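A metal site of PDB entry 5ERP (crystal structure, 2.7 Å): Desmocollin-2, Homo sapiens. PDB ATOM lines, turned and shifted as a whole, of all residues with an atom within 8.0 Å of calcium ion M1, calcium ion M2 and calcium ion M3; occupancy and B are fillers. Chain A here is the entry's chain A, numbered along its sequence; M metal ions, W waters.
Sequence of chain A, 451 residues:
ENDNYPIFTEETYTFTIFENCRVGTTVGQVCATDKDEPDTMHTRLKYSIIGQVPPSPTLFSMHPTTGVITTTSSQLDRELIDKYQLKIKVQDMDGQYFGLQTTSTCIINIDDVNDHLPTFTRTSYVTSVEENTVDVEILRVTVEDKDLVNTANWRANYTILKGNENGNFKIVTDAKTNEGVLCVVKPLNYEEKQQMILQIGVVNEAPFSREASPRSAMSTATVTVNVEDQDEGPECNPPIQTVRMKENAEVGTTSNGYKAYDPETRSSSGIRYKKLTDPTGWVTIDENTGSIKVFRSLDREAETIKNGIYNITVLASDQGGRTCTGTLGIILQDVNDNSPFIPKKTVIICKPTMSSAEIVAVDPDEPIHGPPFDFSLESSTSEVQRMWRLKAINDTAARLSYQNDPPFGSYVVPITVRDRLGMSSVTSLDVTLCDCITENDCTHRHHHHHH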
ATOM      1  N   GLU A 131       1.013  18.108 -14.355  1.00  0.00           N
ATOM      2  CA  GLU A 131      -0.099  17.154 -14.473  1.00  0.00           C
ATOM      3  C   GLU A 131      -1.452  17.856 -14.408  1.00  0.00           C
ATOM      4  O   GLU A 131      -1.550  19.001 -13.971  1.00  0.00           O
ATOM      5  CB  GLU A 131      -0.010  16.093 -13.369  1.00  0.00           C
ATOM      6  CG  GLU A 131      -0.241  16.632 -11.965  1.00  0.00           C
ATOM      7  CD  GLU A 131      -0.257  15.534 -10.926  1.00  0.00           C
ATOM      8  OE1 GLU A 131      -0.810  14.451 -11.216  1.00  0.00           O
ATOM      9  OE2 GLU A 131       0.294  15.754  -9.835  1.00  0.00           O
ATOM     10  N   ASN A 132      -2.490  17.149 -14.860  1.00  0.00           N
ATOM     11  CA  ASN A 132      -3.849  17.670 -14.860  1.00  0.00           C
ATOM     12  C   ASN A 132      -3.934  19.013 -15.574  1.00  0.00           C
ATOM     13  O   ASN A 132      -4.790  19.840 -15.284  1.00  0.00           O
ATOM     14  CB  ASN A 132      -4.361  17.804 -13.426  1.00  0.00           C
ATOM     15  CG  ASN A 132      -4.389  16.477 -12.698  1.00  0.00           C
ATOM     16  OD1 ASN A 132      -4.940  15.498 -13.192  1.00  0.00           O
ATOM     17  ND2 ASN A 132      -3.750  16.432 -11.534  1.00  0.00           N
ATOM     18  N   LEU A 188      -2.310  14.722 -18.007  1.00  0.00           N
ATOM     19  CA  LEU A 188      -1.446  13.645 -17.556  1.00  0.00           C
ATOM     20  C   LEU A 188      -1.569  13.500 -16.050  1.00  0.00           C
ATOM     21  O   LEU A 188      -2.022  14.413 -15.371  1.00  0.00           O
ATOM     22  CB  LEU A 188      -0.001  13.920 -17.964  1.00  0.00           C
ATOM     23  CG  LEU A 188       0.180  14.124 -19.475  1.00  0.00           C
ATOM     24  CD1 LEU A 188       1.462  14.871 -19.785  1.00  0.00           C
ATOM     25  CD2 LEU A 188       0.165  12.771 -20.179  1.00  0.00           C
ATOM     26  N   ASN A 189      -1.164  12.339 -15.544  1.00  0.00           N
ATOM     27  CA  ASN A 189      -1.262  12.053 -14.123  1.00  0.00           C
ATOM     28  C   ASN A 189       0.063  11.539 -13.587  1.00  0.00           C
ATOM     29  O   ASN A 189       0.452  10.413 -13.879  1.00  0.00           O
ATOM     30  CB  ASN A 189      -2.370  11.024 -13.869  1.00  0.00           C
ATOM     31  CG  ASN A 189      -2.799  10.985 -12.418  1.00  0.00           C
ATOM     32  OD1 ASN A 189      -2.909  12.022 -11.776  1.00  0.00           O
ATOM     33  ND2 ASN A 189      -3.020   9.796 -11.886  1.00  0.00           N
ATOM     34  N   TYR A 190       0.755  12.370 -12.813  1.00  0.00           N
ATOM     35  CA  TYR A 190       2.074  12.017 -12.299  1.00  0.00           C
ATOM     36  C   TYR A 190       2.056  10.679 -11.547  1.00  0.00           C
ATOM     37  O   TYR A 190       3.083  10.015 -11.432  1.00  0.00           O
ATOM     38  CB  TYR A 190       2.611  13.116 -11.392  1.00  0.00           C
ATOM     39  CG  TYR A 190       3.930  12.781 -10.728  1.00  0.00           C
ATOM     40  CD1 TYR A 190       5.135  12.966 -11.385  1.00  0.00           C
ATOM     41  CD2 TYR A 190       3.965  12.264  -9.429  1.00  0.00           C
ATOM     42  CE1 TYR A 190       6.340  12.648 -10.790  1.00  0.00           C
ATOM     43  CE2 TYR A 190       5.161  11.944  -8.823  1.00  0.00           C
ATOM     44  CZ  TYR A 190       6.348  12.135  -9.503  1.00  0.00           C
ATOM     45  OH  TYR A 190       7.547  11.825  -8.910  1.00  0.00           O
ATOM     46  N   GLU A 191       0.890  10.296 -11.033  1.00  0.00           N
ATOM     47  CA  GLU A 191       0.789   9.091 -10.225  1.00  0.00           C
ATOM     48  C   GLU A 191       0.694   7.818 -11.066  1.00  0.00           C
ATOM     49  O   GLU A 191       0.994   6.730 -10.583  1.00  0.00           O
ATOM     50  CB  GLU A 191      -0.424   9.194  -9.303  1.00  0.00           C
ATOM     51  CG  GLU A 191      -0.158  10.041  -8.065  1.00  0.00           C
ATOM     52  CD  GLU A 191      -0.238  11.538  -8.333  1.00  0.00           C
ATOM     53  OE1 GLU A 191       0.351  12.308  -7.544  1.00  0.00           O
ATOM     54  OE2 GLU A 191      -0.860  11.945  -9.334  1.00  0.00           O
ATOM     55  N   GLU A 192       0.289   7.962 -12.324  1.00  0.00           N
ATOM     56  CA  GLU A 192       0.270   6.835 -13.255  1.00  0.00           C
ATOM     57  C   GLU A 192       1.614   6.739 -13.969  1.00  0.00           C
ATOM     58  O   GLU A 192       2.279   5.701 -13.927  1.00  0.00           O
ATOM     59  CB  GLU A 192      -0.853   6.979 -14.268  1.00  0.00           C
ATOM     60  CG  GLU A 192      -0.916   5.846 -15.291  1.00  0.00           C
ATOM     61  CD  GLU A 192      -2.086   5.966 -16.237  1.00  0.00           C
ATOM     62  OE1 GLU A 192      -2.275   5.049 -17.071  1.00  0.00           O
ATOM     63  OE2 GLU A 192      -2.811   6.975 -16.159  1.00  0.00           O
ATOM     64  N   VAL A 227       6.584  14.478 -16.484  1.00  0.00           N
ATOM     65  CA  VAL A 227       5.385  15.001 -15.840  1.00  0.00           C
ATOM     66  C   VAL A 227       5.731  15.569 -14.473  1.00  0.00           C
ATOM     67  O   VAL A 227       6.461  14.945 -13.712  1.00  0.00           O
ATOM     68  CB  VAL A 227       4.309  13.913 -15.693  1.00  0.00           C
ATOM     69  CG1 VAL A 227       3.031  14.509 -15.132  1.00  0.00           C
ATOM     70  CG2 VAL A 227       4.037  13.231 -17.028  1.00  0.00           C
ATOM     71  N   GLU A 228       5.219  16.763 -14.182  1.00  0.00           N
ATOM     72  CA  GLU A 228       5.424  17.395 -12.877  1.00  0.00           C
ATOM     73  C   GLU A 228       4.300  17.065 -11.920  1.00  0.00           C
ATOM     74  O   GLU A 228       3.122  17.059 -12.293  1.00  0.00           O
ATOM     75  CB  GLU A 228       5.554  18.911 -12.990  1.00  0.00           C
ATOM     76  CG  GLU A 228       6.948  19.419 -13.275  1.00  0.00           C
ATOM     77  CD  GLU A 228       7.021  20.932 -13.224  1.00  0.00           C
ATOM     78  OE1 GLU A 228       6.149  21.594 -13.832  1.00  0.00           O
ATOM     79  OE2 GLU A 228       7.946  21.464 -12.571  1.00  0.00           O
ATOM     80  N   ASP A 229       4.672  16.799 -10.671  1.00  0.00           N
ATOM     81  CA  ASP A 229       3.727  16.487  -9.622  1.00  0.00           C
ATOM     82  C   ASP A 229       3.057  17.750  -9.073  1.00  0.00           C
ATOM     83  O   ASP A 229       3.742  18.724  -8.730  1.00  0.00           O
ATOM     84  CB  ASP A 229       4.440  15.723  -8.493  1.00  0.00           C
ATOM     85  CG  ASP A 229       3.489  15.232  -7.417  1.00  0.00           C
ATOM     86  OD1 ASP A 229       2.264  15.307  -7.616  1.00  0.00           O
ATOM     87  OD2 ASP A 229       3.980  14.780  -6.365  1.00  0.00           O
ATOM     88  N   GLN A 230       1.731  17.726  -8.999  1.00  0.00           N
ATOM     89  CA  GLN A 230       0.968  18.733  -8.279  1.00  0.00           C
ATOM     90  C   GLN A 230       0.527  18.179  -6.939  1.00  0.00           C
ATOM     91  O   GLN A 230       0.117  17.024  -6.855  1.00  0.00           O
ATOM     92  CB  GLN A 230      -0.286  19.151  -9.058  1.00  0.00           C
ATOM     93  CG  GLN A 230      -0.091  20.097 -10.219  1.00  0.00           C
ATOM     94  CD  GLN A 230      -1.420  20.455 -10.868  1.00  0.00           C
ATOM     95  OE1 GLN A 230      -2.403  19.714 -10.741  1.00  0.00           O
ATOM     96  NE2 GLN A 230      -1.460  21.596 -11.537  1.00  0.00           N
ATOM     97  N   ASP A 231       0.592  19.002  -5.894  1.00  0.00           N
ATOM     98  CA  ASP A 231       0.079  18.598  -4.595  1.00  0.00           C
ATOM     99  C   ASP A 231      -1.445  18.610  -4.680  1.00  0.00           C
ATOM    100  O   ASP A 231      -2.079  19.651  -4.567  1.00  0.00           O
ATOM    101  CB  ASP A 231       0.578  19.533  -3.490  1.00  0.00           C
ATOM    102  CG  ASP A 231       0.120  19.113  -2.113  1.00  0.00           C
ATOM    103  OD1 ASP A 231      -0.397  17.993  -1.968  1.00  0.00           O
ATOM    104  OD2 ASP A 231       0.290  19.914  -1.164  1.00  0.00           O
ATOM    105  N   GLU A 232      -2.030  17.426  -4.871  1.00  0.00           N
ATOM    106  CA  GLU A 232      -3.471  17.311  -5.076  1.00  0.00           C
ATOM    107  C   GLU A 232      -4.214  17.015  -3.779  1.00  0.00           C
ATOM    108  O   GLU A 232      -3.623  16.638  -2.776  1.00  0.00           O
ATOM    109  CB  GLU A 232      -3.771  16.217  -6.114  1.00  0.00           C
ATOM    110  CG  GLU A 232      -3.279  16.556  -7.510  1.00  0.00           C
ATOM    111  CD  GLU A 232      -3.199  15.335  -8.393  1.00  0.00           C
ATOM    112  OE1 GLU A 232      -2.234  14.565  -8.251  1.00  0.00           O
ATOM    113  OE2 GLU A 232      -4.108  15.163  -9.234  1.00  0.00           O
ATOM    114  N   GLY A 233      -5.532  17.182  -3.828  1.00  0.00           N
ATOM    115  CA  GLY A 233      -6.388  16.979  -2.683  1.00  0.00           C
ATOM    116  C   GLY A 233      -6.826  15.538  -2.512  1.00  0.00           C
ATOM    117  O   GLY A 233      -6.405  14.675  -3.288  1.00  0.00           O
ATOM    118  N   PRO A 234      -7.682  15.278  -1.528  1.00  0.00           N
ATOM    119  CA  PRO A 234      -8.109  13.923  -1.163  1.00  0.00           C
ATOM    120  C   PRO A 234      -8.850  13.228  -2.296  1.00  0.00           C
ATOM    121  O   PRO A 234      -9.543  13.889  -3.056  1.00  0.00           O
ATOM    122  CB  PRO A 234      -9.026  14.149   0.043  1.00  0.00           C
ATOM    123  CG  PRO A 234      -9.548  15.522  -0.138  1.00  0.00           C
ATOM    124  CD  PRO A 234      -8.436  16.298  -0.780  1.00  0.00           C
ATOM    125  N   GLU A 235      -8.681  11.906  -2.394  1.00  0.00           N
ATOM    126  CA  GLU A 235      -9.333  11.122  -3.439  1.00  0.00           C
ATOM    127  C   GLU A 235     -10.278  10.098  -2.841  1.00  0.00           C
ATOM    128  O   GLU A 235      -9.922   9.399  -1.881  1.00  0.00           O
ATOM    129  CB  GLU A 235      -8.258  10.423  -4.297  1.00  0.00           C
ATOM    130  CG  GLU A 235      -8.796   9.564  -5.434  1.00  0.00           C
ATOM    131  CD  GLU A 235      -7.691   8.971  -6.289  1.00  0.00           C
ATOM    132  OE1 GLU A 235      -6.500   9.228  -6.003  1.00  0.00           O
ATOM    133  OE2 GLU A 235      -8.005   8.232  -7.247  1.00  0.00           O
ATOM    134  N   TYR A 261      -8.008   9.137   0.732  1.00  0.00           N
ATOM    135  CA  TYR A 261      -6.570   9.231   0.911  1.00  0.00           C
ATOM    136  C   TYR A 261      -5.956  10.336   0.058  1.00  0.00           C
ATOM    137  O   TYR A 261      -6.588  10.813  -0.890  1.00  0.00           O
ATOM    138  CB  TYR A 261      -5.914   7.889   0.590  1.00  0.00           C
ATOM    139  CG  TYR A 261      -6.163   7.385  -0.813  1.00  0.00           C
ATOM    140  CD1 TYR A 261      -5.391   7.825  -1.878  1.00  0.00           C
ATOM    141  CD2 TYR A 261      -7.171   6.459  -1.071  1.00  0.00           C
ATOM    142  CE1 TYR A 261      -5.611   7.362  -3.157  1.00  0.00           C
ATOM    143  CE2 TYR A 261      -7.404   6.000  -2.350  1.00  0.00           C
ATOM    144  CZ  TYR A 261      -6.625   6.452  -3.388  1.00  0.00           C
ATOM    145  OH  TYR A 261      -6.850   5.998  -4.669  1.00  0.00           O
ATOM    146  N   ASP A 262      -4.744  10.747   0.406  1.00  0.00           N
ATOM    147  CA  ASP A 262      -4.005  11.718  -0.388  1.00  0.00           C
ATOM    148  C   ASP A 262      -3.307  10.989  -1.536  1.00  0.00           C
ATOM    149  O   ASP A 262      -2.694   9.943  -1.316  1.00  0.00           O
ATOM    150  CB  ASP A 262      -2.987  12.460   0.499  1.00  0.00           C
ATOM    151  CG  ASP A 262      -2.353  13.644  -0.209  1.00  0.00           C
ATOM    152  OD1 ASP A 262      -3.056  14.319  -0.984  1.00  0.00           O
ATOM    153  OD2 ASP A 262      -1.158  13.902   0.025  1.00  0.00           O
ATOM    154  N   PRO A 263      -3.388  11.519  -2.767  1.00  0.00           N
ATOM    155  CA  PRO A 263      -2.745  10.811  -3.890  1.00  0.00           C
ATOM    156  C   PRO A 263      -1.234  10.697  -3.747  1.00  0.00           C
ATOM    157  O   PRO A 263      -0.671   9.671  -4.124  1.00  0.00           O
ATOM    158  CB  PRO A 263      -3.109  11.681  -5.093  1.00  0.00           C
ATOM    159  CG  PRO A 263      -4.360  12.368  -4.701  1.00  0.00           C
ATOM    160  CD  PRO A 263      -4.208  12.654  -3.242  1.00  0.00           C
ATOM    161  N   GLU A 264      -0.581  11.729  -3.213  1.00  0.00           N
ATOM    162  CA  GLU A 264       0.863  11.718  -3.027  1.00  0.00           C
ATOM    163  C   GLU A 264       1.263  10.797  -1.871  1.00  0.00           C
ATOM    164  O   GLU A 264       2.077   9.893  -2.038  1.00  0.00           O
ATOM    165  CB  GLU A 264       1.391  13.128  -2.773  1.00  0.00           C
ATOM    166  CG  GLU A 264       1.268  14.071  -3.960  1.00  0.00           C
ATOM    167  CD  GLU A 264      -0.141  14.584  -4.177  1.00  0.00           C
ATOM    168  OE1 GLU A 264      -0.832  14.875  -3.170  1.00  0.00           O
ATOM    169  OE2 GLU A 264      -0.570  14.690  -5.342  1.00  0.00           O
ATOM    170  N   THR A 265       0.688  11.051  -0.698  1.00  0.00           N
ATOM    171  CA  THR A 265       1.059  10.349   0.522  1.00  0.00           C
ATOM    172  C   THR A 265       0.461   8.948   0.637  1.00  0.00           C
ATOM    173  O   THR A 265       1.028   8.078   1.285  1.00  0.00           O
ATOM    174  CB  THR A 265       0.638  11.149   1.770  1.00  0.00           C
ATOM    175  OG1 THR A 265       1.083  12.509   1.642  1.00  0.00           O
ATOM    176  CG2 THR A 265       1.230  10.542   3.042  1.00  0.00           C
ATOM    177  N   ARG A 266      -0.696   8.747  -0.004  1.00  0.00           N
ATOM    178  CA  ARG A 266      -1.472   7.509   0.136  1.00  0.00           C
ATOM    179  C   ARG A 266      -1.925   7.294   1.583  1.00  0.00           C
ATOM    180  O   ARG A 266      -2.331   6.200   1.961  1.00  0.00           O
ATOM    181  CB  ARG A 266      -0.675   6.284  -0.349  1.00  0.00           C
ATOM    182  CG  ARG A 266      -0.326   6.313  -1.830  1.00  0.00           C
ATOM    183  CD  ARG A 266      -1.523   6.003  -2.723  1.00  0.00           C
ATOM    184  NE  ARG A 266      -2.018   4.638  -2.543  1.00  0.00           N
ATOM    185  CZ  ARG A 266      -2.968   4.087  -3.294  1.00  0.00           C
ATOM    186  NH1 ARG A 266      -3.535   4.778  -4.277  1.00  0.00           N
ATOM    187  NH2 ARG A 266      -3.347   2.836  -3.060  1.00  0.00           N
ATOM    188  N   ASP A 318      -9.304  17.899   3.040  1.00  0.00           N
ATOM    189  CA  ASP A 318      -7.961  17.924   3.588  1.00  0.00           C
ATOM    190  C   ASP A 318      -7.775  19.263   4.279  1.00  0.00           C
ATOM    191  O   ASP A 318      -8.657  20.115   4.240  1.00  0.00           O
ATOM    192  CB  ASP A 318      -6.900  17.701   2.498  1.00  0.00           C
ATOM    193  CG  ASP A 318      -6.892  18.783   1.421  1.00  0.00           C
ATOM    194  OD1 ASP A 318      -7.660  19.770   1.515  1.00  0.00           O
ATOM    195  OD2 ASP A 318      -6.090  18.654   0.478  1.00  0.00           O
ATOM    196  N   ARG A 322      -9.675  21.603   0.125  1.00  0.00           N
ATOM    197  CA  ARG A 322     -10.130  21.011  -1.123  1.00  0.00           C
ATOM    198  C   ARG A 322     -10.821  19.685  -0.833  1.00  0.00           C
ATOM    199  O   ARG A 322     -10.487  18.985   0.127  1.00  0.00           O
ATOM    200  CB  ARG A 322      -8.983  20.840  -2.132  1.00  0.00           C
ATOM    201  CG  ARG A 322      -7.640  20.419  -1.568  1.00  0.00           C
ATOM    202  CD  ARG A 322      -6.549  20.715  -2.568  1.00  0.00           C
ATOM    203  NE  ARG A 322      -5.321  19.974  -2.273  1.00  0.00           N
ATOM    204  CZ  ARG A 322      -4.363  20.391  -1.455  1.00  0.00           C
ATOM    205  NH1 ARG A 322      -4.463  21.564  -0.829  1.00  0.00           N
ATOM    206  NH2 ARG A 322      -3.288  19.644  -1.265  1.00  0.00           N
HETATM  207 CA    CA M   1      -1.600  16.114  -1.260  1.00  0.00          CA
HETATM  208 CA    CA M   2      -2.848  13.276 -10.009  1.00  0.00          CA
HETATM  209 CA    CA M   3      -0.009  14.624  -7.643  1.00  0.00          CA
HETATM  210  O   HOH W   1       0.705  15.976   0.075  1.00  0.00           O
HETATM  211  O   HOH W   2      -4.163  11.558  -8.736  1.00  0.00           O
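OD2 of Asp 262 lies close to OG1 of Thr 265, 3.1 Å away.
OE2 of Glu 232 lies close to ND2 of Asn 132 (2.7 Å).
The backbone NH of Asn 132 sits at hydrogen-bond distance from the backbone carbonyl oxygen of Leu 188.
The guanidinium group (NE) of Arg 322 is in salt-bridge range of the side-chain carboxylate (OD2) of Asp 318, 3.1 Å away.
O of Glu 228 is in hydrogen-bond range of N of Glu 131, 3.1 Å away.
The guanidinium group (NH2) of Arg 322 lies within salt-bridge range of the side-chain carboxylate (OD2) of Asp 231, at 3.6 Å.
The backbone NH (N) of Tyr 190 sits close to the side-chain carboxylate (OE1) of Glu 131 (3.1 Å).
The backbone carbonyl oxygen of Glu 232 sits close to the guanidinium group of Arg 322 (3.4 Å).
Arg 322 touches calcium ion M1 (NH2 to CA, 3.9 Å).
Asn 132 touches calcium ion M2.
Five residues have an atom within 4 Å of calcium ion M2: Glu 131, Asn 132, Asn 189, Glu 191 and Glu 232.
Six residues have an atom within 4 Å of calcium ion M3: Glu 131, Glu 191, Asp 229, Gln 230, Glu 232 and Glu 264.
OD1 of Asp 262 binds calcium ion M1 (2.3 Å).
OD1 of Asp 231 is bound to calcium ion M1.
Calcium ion M1 is bound by OE1 of Glu 264, at 2.4 Å.
Calcium ion M1 is bound by O of Glu 232.
Calcium ion M1 is bound by OD2 of Asp 262.
Water W1 is bound to calcium ion M1 (2.7 Å).
Calcium ion M2 is bound by the side-chain amide oxygen (OD1) of Asn 189 (2.2 Å).
OE1 of Glu 232 is bound to calcium ion M2 (2.3 Å).
OE2 of Glu 232 is bound to calcium ion M2, at 2.4 Å.
OE2 of Glu 191 binds calcium ion M2 (2.5 Å).
Water W2 binds calcium ion M2 (2.5 Å).
OE1 of Glu 131 binds calcium ion M2 (2.6 Å).
Calcium ion M2 has six donor atoms within binding distance.
Calcium ion M3 is bound by OE1 of Glu 232 (2.3 Å), OE1 of Glu 191 (2.3 Å), OE2 of Glu 264 (2.4 Å), OD1 of Asp 229 (2.4 Å), OE2 of Glu 131 (2.5 Å) and O of Gln 230 (2.5 Å).
Calcium ion M3 has six donor atoms within binding distance.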
